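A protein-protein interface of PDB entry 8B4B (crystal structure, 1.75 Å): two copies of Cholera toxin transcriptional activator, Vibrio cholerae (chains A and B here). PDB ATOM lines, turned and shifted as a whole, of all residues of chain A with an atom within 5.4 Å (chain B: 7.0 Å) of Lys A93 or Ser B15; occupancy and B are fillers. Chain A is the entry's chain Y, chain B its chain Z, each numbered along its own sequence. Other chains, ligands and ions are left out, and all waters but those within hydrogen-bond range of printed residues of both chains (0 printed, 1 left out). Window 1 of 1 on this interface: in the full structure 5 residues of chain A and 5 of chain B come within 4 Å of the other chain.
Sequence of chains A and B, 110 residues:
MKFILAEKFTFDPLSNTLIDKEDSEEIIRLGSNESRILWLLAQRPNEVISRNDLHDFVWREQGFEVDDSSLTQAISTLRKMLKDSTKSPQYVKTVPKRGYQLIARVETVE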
ATOM      1  N   ASN A  46      30.624 -27.605  14.652  1.00  0.00           N
ATOM      2  CA  ASN A  46      29.203 -27.725  14.943  1.00  0.00           C
ATOM      3  C   ASN A  46      28.711 -29.163  14.895  1.00  0.00           C
ATOM      4  O   ASN A  46      27.493 -29.396  14.914  1.00  0.00           O
ATOM      5  CB  ASN A  46      28.370 -26.835  14.018  1.00  0.00           C
ATOM      6  CG  ASN A  46      27.096 -26.355  14.674  1.00  0.00           C
ATOM      7  OD1 ASN A  46      27.035 -26.169  15.901  1.00  0.00           O
ATOM      8  ND2 ASN A  46      26.078 -26.119  13.862  1.00  0.00           N
ATOM      9  N   ARG A  79      37.341 -24.455  28.662  1.00  0.00           N
ATOM     10  CA  ARG A  79      36.342 -23.395  28.776  1.00  0.00           C
ATOM     11  C   ARG A  79      36.875 -22.189  29.542  1.00  0.00           C
ATOM     12  O   ARG A  79      36.535 -21.045  29.222  1.00  0.00           O
ATOM     13  CB  ARG A  79      35.066 -23.936  29.440  1.00  0.00           C
ATOM     14  CG  ARG A  79      34.199 -24.742  28.488  1.00  0.00           C
ATOM     15  CD  ARG A  79      32.909 -25.158  29.180  1.00  0.00           C
ATOM     16  NE  ARG A  79      31.960 -25.764  28.266  1.00  0.00           N
ATOM     17  CZ  ARG A  79      31.240 -26.837  28.576  1.00  0.00           C
ATOM     18  NH1 ARG A  79      31.353 -27.423  29.753  1.00  0.00           N
ATOM     19  NH2 ARG A  79      30.408 -27.341  27.679  1.00  0.00           N
ATOM     20  N   PRO A  89      26.908 -21.448  27.078  1.00  0.00           N
ATOM     21  CA  PRO A  89      28.126 -21.600  26.260  1.00  0.00           C
ATOM     22  C   PRO A  89      28.065 -20.802  24.969  1.00  0.00           C
ATOM     23  O   PRO A  89      27.043 -20.760  24.284  1.00  0.00           O
ATOM     24  CB  PRO A  89      28.192 -23.110  25.954  1.00  0.00           C
ATOM     25  CG  PRO A  89      26.981 -23.714  26.531  1.00  0.00           C
ATOM     26  CD  PRO A  89      26.265 -22.724  27.376  1.00  0.00           C
ATOM     27  N   TYR A  91      31.193 -21.275  23.046  1.00  0.00           N
ATOM     28  CA  TYR A  91      32.216 -21.993  22.290  1.00  0.00           C
ATOM     29  C   TYR A  91      31.976 -23.483  22.341  1.00  0.00           C
ATOM     30  O   TYR A  91      31.711 -24.098  21.305  1.00  0.00           O
ATOM     31  CB  TYR A  91      33.609 -21.642  22.814  1.00  0.00           C
ATOM     32  CG  TYR A  91      34.022 -20.216  22.523  1.00  0.00           C
ATOM     33  CD1 TYR A  91      33.680 -19.177  23.386  1.00  0.00           C
ATOM     34  CD2 TYR A  91      34.764 -19.914  21.389  1.00  0.00           C
ATOM     35  CE1 TYR A  91      34.061 -17.873  23.116  1.00  0.00           C
ATOM     36  CE2 TYR A  91      35.149 -18.620  21.113  1.00  0.00           C
ATOM     37  CZ  TYR A  91      34.793 -17.600  21.973  1.00  0.00           C
ATOM     38  OH  TYR A  91      35.184 -16.309  21.688  1.00  0.00           O
ATOM     39  N   VAL A  92      32.050 -24.099  23.517  1.00  0.00           N
ATOM     40  CA  VAL A  92      31.986 -25.548  23.632  1.00  0.00           C
ATOM     41  C   VAL A  92      30.708 -25.883  24.377  1.00  0.00           C
ATOM     42  O   VAL A  92      30.565 -25.536  25.560  1.00  0.00           O
ATOM     43  CB  VAL A  92      33.208 -26.117  24.360  1.00  0.00           C
ATOM     44  CG1 VAL A  92      33.045 -27.614  24.574  1.00  0.00           C
ATOM     45  CG2 VAL A  92      34.500 -25.781  23.612  1.00  0.00           C
ATOM     46  N   LYS A  93      29.814 -26.587  23.714  1.00  0.00           N
ATOM     47  CA  LYS A  93      28.546 -26.963  24.318  1.00  0.00           C
ATOM     48  C   LYS A  93      28.545 -28.437  24.691  1.00  0.00           C
ATOM     49  O   LYS A  93      29.019 -29.291  23.936  1.00  0.00           O
ATOM     50  CB  LYS A  93      27.387 -26.643  23.380  1.00  0.00           C
ATOM     51  CG  LYS A  93      26.025 -27.092  23.907  1.00  0.00           C
ATOM     52  CD  LYS A  93      24.891 -26.463  23.118  1.00  0.00           C
ATOM     53  CE  LYS A  93      24.470 -27.332  21.955  1.00  0.00           C
ATOM     54  NZ  LYS A  93      24.460 -26.606  20.657  1.00  0.00           N
ATOM     55  N   THR A  94      28.005 -28.733  25.867  1.00  0.00           N
ATOM     56  CA  THR A  94      27.877 -30.124  26.294  1.00  0.00           C
ATOM     57  C   THR A  94      26.600 -30.710  25.717  1.00  0.00           C
ATOM     58  O   THR A  94      25.542 -30.055  25.731  1.00  0.00           O
ATOM     59  CB  THR A  94      27.876 -30.211  27.831  1.00  0.00           C
ATOM     60  OG1 THR A  94      29.116 -29.688  28.314  1.00  0.00           O
ATOM     61  CG2 THR A  94      27.722 -31.653  28.271  1.00  0.00           C
ATOM     62  N   VAL A  95      26.703 -31.921  25.166  1.00  0.00           N
ATOM     63  CA  VAL A  95      25.544 -32.640  24.659  1.00  0.00           C
ATOM     64  C   VAL A  95      25.362 -33.894  25.503  1.00  0.00           C
ATOM     65  O   VAL A  95      25.941 -34.951  25.195  1.00  0.00           O
ATOM     66  CB  VAL A  95      25.674 -32.967  23.162  1.00  0.00           C
ATOM     67  CG1 VAL A  95      24.346 -33.450  22.646  1.00  0.00           C
ATOM     68  CG2 VAL A  95      26.102 -31.709  22.386  1.00  0.00           C
ATOM     69  N   GLY A  99      28.280 -36.333  24.040  1.00  0.00           N
ATOM     70  CA  GLY A  99      29.613 -35.743  23.885  1.00  0.00           C
ATOM     71  C   GLY A  99      29.694 -34.230  24.021  1.00  0.00           C
ATOM     72  O   GLY A  99      29.128 -33.663  24.959  1.00  0.00           O
ATOM     73  N   TYR A 100      30.439 -33.564  23.132  1.00  0.00           N
ATOM     74  CA  TYR A 100      30.603 -32.111  23.154  1.00  0.00           C
ATOM     75  C   TYR A 100      30.565 -31.604  21.720  1.00  0.00           C
ATOM     76  O   TYR A 100      30.812 -32.362  20.779  1.00  0.00           O
ATOM     77  CB  TYR A 100      31.920 -31.679  23.811  1.00  0.00           C
ATOM     78  CG  TYR A 100      32.028 -32.042  25.282  1.00  0.00           C
ATOM     79  CD1 TYR A 100      31.572 -31.185  26.280  1.00  0.00           C
ATOM     80  CD2 TYR A 100      32.581 -33.254  25.667  1.00  0.00           C
ATOM     81  CE1 TYR A 100      31.677 -31.534  27.618  1.00  0.00           C
ATOM     82  CE2 TYR A 100      32.674 -33.610  26.974  1.00  0.00           C
ATOM     83  CZ  TYR A 100      32.243 -32.754  27.947  1.00  0.00           C
ATOM     84  OH  TYR A 100      32.371 -33.124  29.263  1.00  0.00           O
ATOM     85  N   GLN A 101      30.278 -30.308  21.564  1.00  0.00           N
ATOM     86  CA  GLN A 101      29.992 -29.716  20.257  1.00  0.00           C
ATOM     87  C   GLN A 101      30.555 -28.301  20.217  1.00  0.00           C
ATOM     88  O   GLN A 101      30.226 -27.482  21.082  1.00  0.00           O
ATOM     89  CB  GLN A 101      28.472 -29.719  20.006  1.00  0.00           C
ATOM     90  CG  GLN A 101      28.016 -29.112  18.675  1.00  0.00           C
ATOM     91  CD  GLN A 101      26.497 -28.957  18.625  1.00  0.00           C
ATOM     92  OE1 GLN A 101      25.809 -29.126  19.639  1.00  0.00           O
ATOM     93  NE2 GLN A 101      25.971 -28.641  17.446  1.00  0.00           N
ATOM     94  N   LEU A 102      31.405 -28.003  19.230  1.00  0.00           N
ATOM     95  CA  LEU A 102      31.943 -26.653  19.102  1.00  0.00           C
ATOM     96  C   LEU A 102      30.921 -25.824  18.333  1.00  0.00           C
ATOM     97  O   LEU A 102      30.689 -26.045  17.132  1.00  0.00           O
ATOM     98  CB  LEU A 102      33.310 -26.674  18.411  1.00  0.00           C
ATOM     99  CG  LEU A 102      34.028 -25.331  18.197  1.00  0.00           C
ATOM    100  CD1 LEU A 102      34.240 -24.557  19.507  1.00  0.00           C
ATOM    101  CD2 LEU A 102      35.383 -25.600  17.540  1.00  0.00           C
ATOM    102  N   ILE A 103      30.273 -24.887  19.025  1.00  0.00           N
ATOM    103  CA  ILE A 103      29.227 -24.086  18.405  1.00  0.00           C
ATOM    104  C   ILE A 103      29.713 -22.719  17.942  1.00  0.00           C
ATOM    105  O   ILE A 103      28.965 -22.019  17.244  1.00  0.00           O
ATOM    106  CB  ILE A 103      28.030 -23.934  19.363  1.00  0.00           C
ATOM    107  CG1 ILE A 103      28.487 -23.293  20.685  1.00  0.00           C
ATOM    108  CG2 ILE A 103      27.360 -25.276  19.560  1.00  0.00           C
ATOM    109  CD1 ILE A 103      27.321 -22.838  21.588  1.00  0.00           C
ATOM    110  N   PHE B  11      13.744 -23.271  14.463  1.00  0.00           N
ATOM    111  CA  PHE B  11      14.132 -24.490  15.166  1.00  0.00           C
ATOM    112  C   PHE B  11      15.324 -25.103  14.448  1.00  0.00           C
ATOM    113  O   PHE B  11      15.232 -25.443  13.264  1.00  0.00           O
ATOM    114  CB  PHE B  11      12.961 -25.477  15.217  1.00  0.00           C
ATOM    115  CG  PHE B  11      13.338 -26.862  15.676  1.00  0.00           C
ATOM    116  CD1 PHE B  11      14.154 -27.049  16.785  1.00  0.00           C
ATOM    117  CD2 PHE B  11      12.852 -27.978  15.009  1.00  0.00           C
ATOM    118  CE1 PHE B  11      14.486 -28.330  17.207  1.00  0.00           C
ATOM    119  CE2 PHE B  11      13.182 -29.261  15.419  1.00  0.00           C
ATOM    120  CZ  PHE B  11      14.000 -29.438  16.518  1.00  0.00           C
ATOM    121  N   ASP B  12      16.433 -25.248  15.164  1.00  0.00           N
ATOM    122  CA  ASP B  12      17.604 -25.921  14.613  1.00  0.00           C
ATOM    123  C   ASP B  12      17.819 -27.237  15.350  1.00  0.00           C
ATOM    124  O   ASP B  12      18.269 -27.223  16.507  1.00  0.00           O
ATOM    125  CB  ASP B  12      18.842 -25.031  14.738  1.00  0.00           C
ATOM    126  CG  ASP B  12      20.064 -25.632  14.068  1.00  0.00           C
ATOM    127  OD1 ASP B  12      20.024 -26.814  13.642  1.00  0.00           O
ATOM    128  OD2 ASP B  12      21.071 -24.903  13.962  1.00  0.00           O
ATOM    129  N   PRO B  13      17.518 -28.388  14.736  1.00  0.00           N
ATOM    130  CA  PRO B  13      17.649 -29.658  15.461  1.00  0.00           C
ATOM    131  C   PRO B  13      19.090 -30.096  15.607  1.00  0.00           C
ATOM    132  O   PRO B  13      19.373 -30.999  16.408  1.00  0.00           O
ATOM    133  CB  PRO B  13      16.867 -30.652  14.594  1.00  0.00           C
ATOM    134  CG  PRO B  13      16.806 -30.045  13.235  1.00  0.00           C
ATOM    135  CD  PRO B  13      17.074 -28.567  13.343  1.00  0.00           C
ATOM    136  N   LEU B  14      19.999 -29.490  14.846  1.00  0.00           N
ATOM    137  CA  LEU B  14      21.417 -29.788  14.968  1.00  0.00           C
ATOM    138  C   LEU B  14      22.047 -29.077  16.159  1.00  0.00           C
ATOM    139  O   LEU B  14      23.107 -29.504  16.630  1.00  0.00           O
ATOM    140  CB  LEU B  14      22.123 -29.407  13.664  1.00  0.00           C
ATOM    141  CG  LEU B  14      21.517 -30.077  12.420  1.00  0.00           C
ATOM    142  CD1 LEU B  14      22.343 -29.805  11.174  1.00  0.00           C
ATOM    143  CD2 LEU B  14      21.343 -31.579  12.614  1.00  0.00           C
ATOM    144  N   SER B  15      21.404 -28.026  16.671  1.00  0.00           N
ATOM    145  CA  SER B  15      21.877 -27.297  17.838  1.00  0.00           C
ATOM    146  C   SER B  15      20.918 -27.381  19.022  1.00  0.00           C
ATOM    147  O   SER B  15      21.195 -26.771  20.057  1.00  0.00           O
ATOM    148  CB  SER B  15      22.105 -25.820  17.480  1.00  0.00           C
ATOM    149  OG  SER B  15      22.788 -25.676  16.239  1.00  0.00           O
ATOM    150  N   ASN B  16      19.790 -28.092  18.886  1.00  0.00           N
ATOM    151  CA  ASN B  16      18.752 -28.177  19.923  1.00  0.00           C
ATOM    152  C   ASN B  16      18.318 -26.793  20.404  1.00  0.00           C
ATOM    153  O   ASN B  16      18.231 -26.533  21.605  1.00  0.00           O
ATOM    154  CB  ASN B  16      19.219 -29.012  21.121  1.00  0.00           C
ATOM    155  CG  ASN B  16      19.450 -30.461  20.773  1.00  0.00           C
ATOM    156  OD1 ASN B  16      19.136 -30.906  19.671  1.00  0.00           O
ATOM    157  ND2 ASN B  16      19.991 -31.211  21.720  1.00  0.00           N
ATOM    158  N   THR B  17      18.029 -25.889  19.468  1.00  0.00           N
ATOM    159  CA  THR B  17      17.674 -24.534  19.862  1.00  0.00           C
ATOM    160  C   THR B  17      16.388 -24.058  19.199  1.00  0.00           C
ATOM    161  O   THR B  17      16.035 -24.457  18.079  1.00  0.00           O
ATOM    162  CB  THR B  17      18.797 -23.523  19.550  1.00  0.00           C
ATOM    163  OG1 THR B  17      19.038 -23.508  18.134  1.00  0.00           O
ATOM    164  CG2 THR B  17      20.071 -23.865  20.320  1.00  0.00           C
ATOM    165  N   LEU B  18      15.718 -23.167  19.921  1.00  0.00           N
ATOM    166  CA  LEU B  18      14.524 -22.468  19.486  1.00  0.00           C
ATOM    167  C   LEU B  18      14.817 -20.977  19.618  1.00  0.00           C
ATOM    168  O   LEU B  18      15.313 -20.538  20.660  1.00  0.00           O
ATOM    169  CB  LEU B  18      13.348 -22.868  20.379  1.00  0.00           C
ATOM    170  CG  LEU B  18      12.436 -24.056  20.056  1.00  0.00           C
ATOM    171  CD1 LEU B  18      11.186 -23.958  20.909  1.00  0.00           C
ATOM    172  CD2 LEU B  18      12.082 -24.177  18.575  1.00  0.00           C
ATOM    173  N   ILE B  27      18.086 -17.246  22.957  1.00  0.00           N
ATOM    174  CA  ILE B  27      18.014 -18.637  22.529  1.00  0.00           C
ATOM    175  C   ILE B  27      17.284 -19.452  23.586  1.00  0.00           C
ATOM    176  O   ILE B  27      17.557 -19.332  24.788  1.00  0.00           O
ATOM    177  CB  ILE B  27      19.416 -19.208  22.275  1.00  0.00           C
ATOM    178  CG1 ILE B  27      20.065 -18.529  21.068  1.00  0.00           C
ATOM    179  CG2 ILE B  27      19.349 -20.720  22.117  1.00  0.00           C
ATOM    180  CD1 ILE B  27      21.080 -19.398  20.355  1.00  0.00           C
ATOM    181  N   ILE B  28      16.356 -20.289  23.140  1.00  0.00           N
ATOM    182  CA  ILE B  28      15.684 -21.255  23.998  1.00  0.00           C
ATOM    183  C   ILE B  28      16.383 -22.594  23.797  1.00  0.00           C
ATOM    184  O   ILE B  28      16.409 -23.130  22.684  1.00  0.00           O
ATOM    185  CB  ILE B  28      14.188 -21.322  23.676  1.00  0.00           C
ATOM    186  CG1 ILE B  28      13.531 -19.971  23.974  1.00  0.00           C
ATOM    187  CG2 ILE B  28      13.519 -22.454  24.428  1.00  0.00           C
ATOM    188  CD1 ILE B  28      12.210 -19.758  23.282  1.00  0.00           C
ATOM    189  N   ARG B  29      16.992 -23.122  24.862  1.00  0.00           N
ATOM    190  CA  ARG B  29      17.781 -24.342  24.744  1.00  0.00           C
ATOM    191  C   ARG B  29      16.887 -25.549  25.019  1.00  0.00           C
ATOM    192  O   ARG B  29      16.309 -25.673  26.104  1.00  0.00           O
ATOM    193  CB  ARG B  29      18.979 -24.311  25.694  1.00  0.00           C
ATOM    194  CG  ARG B  29      19.782 -23.007  25.647  1.00  0.00           C
ATOM    195  CD  ARG B  29      21.308 -23.177  25.599  1.00  0.00           C
ATOM    196  NE  ARG B  29      21.823 -23.214  24.231  1.00  0.00           N
ATOM    197  CZ  ARG B  29      23.086 -22.978  23.893  1.00  0.00           C
ATOM    198  NH1 ARG B  29      23.996 -22.656  24.798  1.00  0.00           N
ATOM    199  NH2 ARG B  29      23.440 -23.044  22.610  1.00  0.00           N
ATOM    200  N   LEU B  30      16.765 -26.430  24.033  1.00  0.00           N
ATOM    201  CA  LEU B  30      15.989 -27.655  24.168  1.00  0.00           C
ATOM    202  C   LEU B  30      16.892 -28.793  24.617  1.00  0.00           C
ATOM    203  O   LEU B  30      18.037 -28.903  24.173  1.00  0.00           O
ATOM    204  CB  LEU B  30      15.333 -28.032  22.831  1.00  0.00           C
ATOM    205  CG  LEU B  30      14.107 -27.241  22.357  1.00  0.00           C
ATOM    206  CD1 LEU B  30      13.527 -27.899  21.123  1.00  0.00           C
ATOM    207  CD2 LEU B  30      13.047 -27.146  23.439  1.00  0.00           C
ATOM    208  N   SER B  35      14.065 -31.964  21.529  1.00  0.00           N
ATOM    209  CA  SER B  35      14.450 -31.566  20.181  1.00  0.00           C
ATOM    210  C   SER B  35      14.210 -32.699  19.171  1.00  0.00           C
ATOM    211  O   SER B  35      13.732 -32.460  18.058  1.00  0.00           O
ATOM    212  CB  SER B  35      15.927 -31.102  20.203  1.00  0.00           C
ATOM    213  OG  SER B  35      16.353 -30.684  18.914  1.00  0.00           O
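O of Ser B15 lies within hydrogen-bond range of NZ of Lys A93. The backbone carbonyl oxygen (O) of Leu B14 sits at hydrogen-bond distance from the side-chain amide nitrogen (NE2) of Gln A101 (3.1 Å).
O of Asn A46 lies within hydrogen-bond range of NE2 of Gln A101. The backbone NH (N) of Lys A93 is in hydrogen-bond range of the backbone carbonyl oxygen (O) of Gln A101. N of Leu B14 is in hydrogen-bond range of OD1 of Asp B12 (2.9 Å). The side-chain carboxylate (OD2) of Asp B12 is in hydrogen-bond range of the side-chain hydroxyl (OG) of Ser B15.
Among the printed residues, merely in contact across the chains: Pro A89 with Arg B29 (3.4 Å) and Lys A93 with Arg B29 (3.7 Å).
Printed residues of chain A within 4 Å of Ser B15: Lys A93 (3.3 Å). Printed residues of chain A within 4 Å of Leu B14: Gln A101. Of the printed residues of chain B, Gln A101 touches Leu B14. Printed residues of chain B within 4 Å of Pro A89: Arg B29. Val A95 touches none of the printed residues of chain B. Arg A79 touches none of the printed residues of chain B. The nearest residue of chain A that does not touch Ser B15 is Asn A46 (4.1 Å).
Hydrophobic or aromatic side chains of chain A that line the printed part of chain B: Pro A89.
No position is printed for both chains. Of the 4 pairs that touch across the chains among the printed residues, none has its exchanged pair printed and touching as well.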
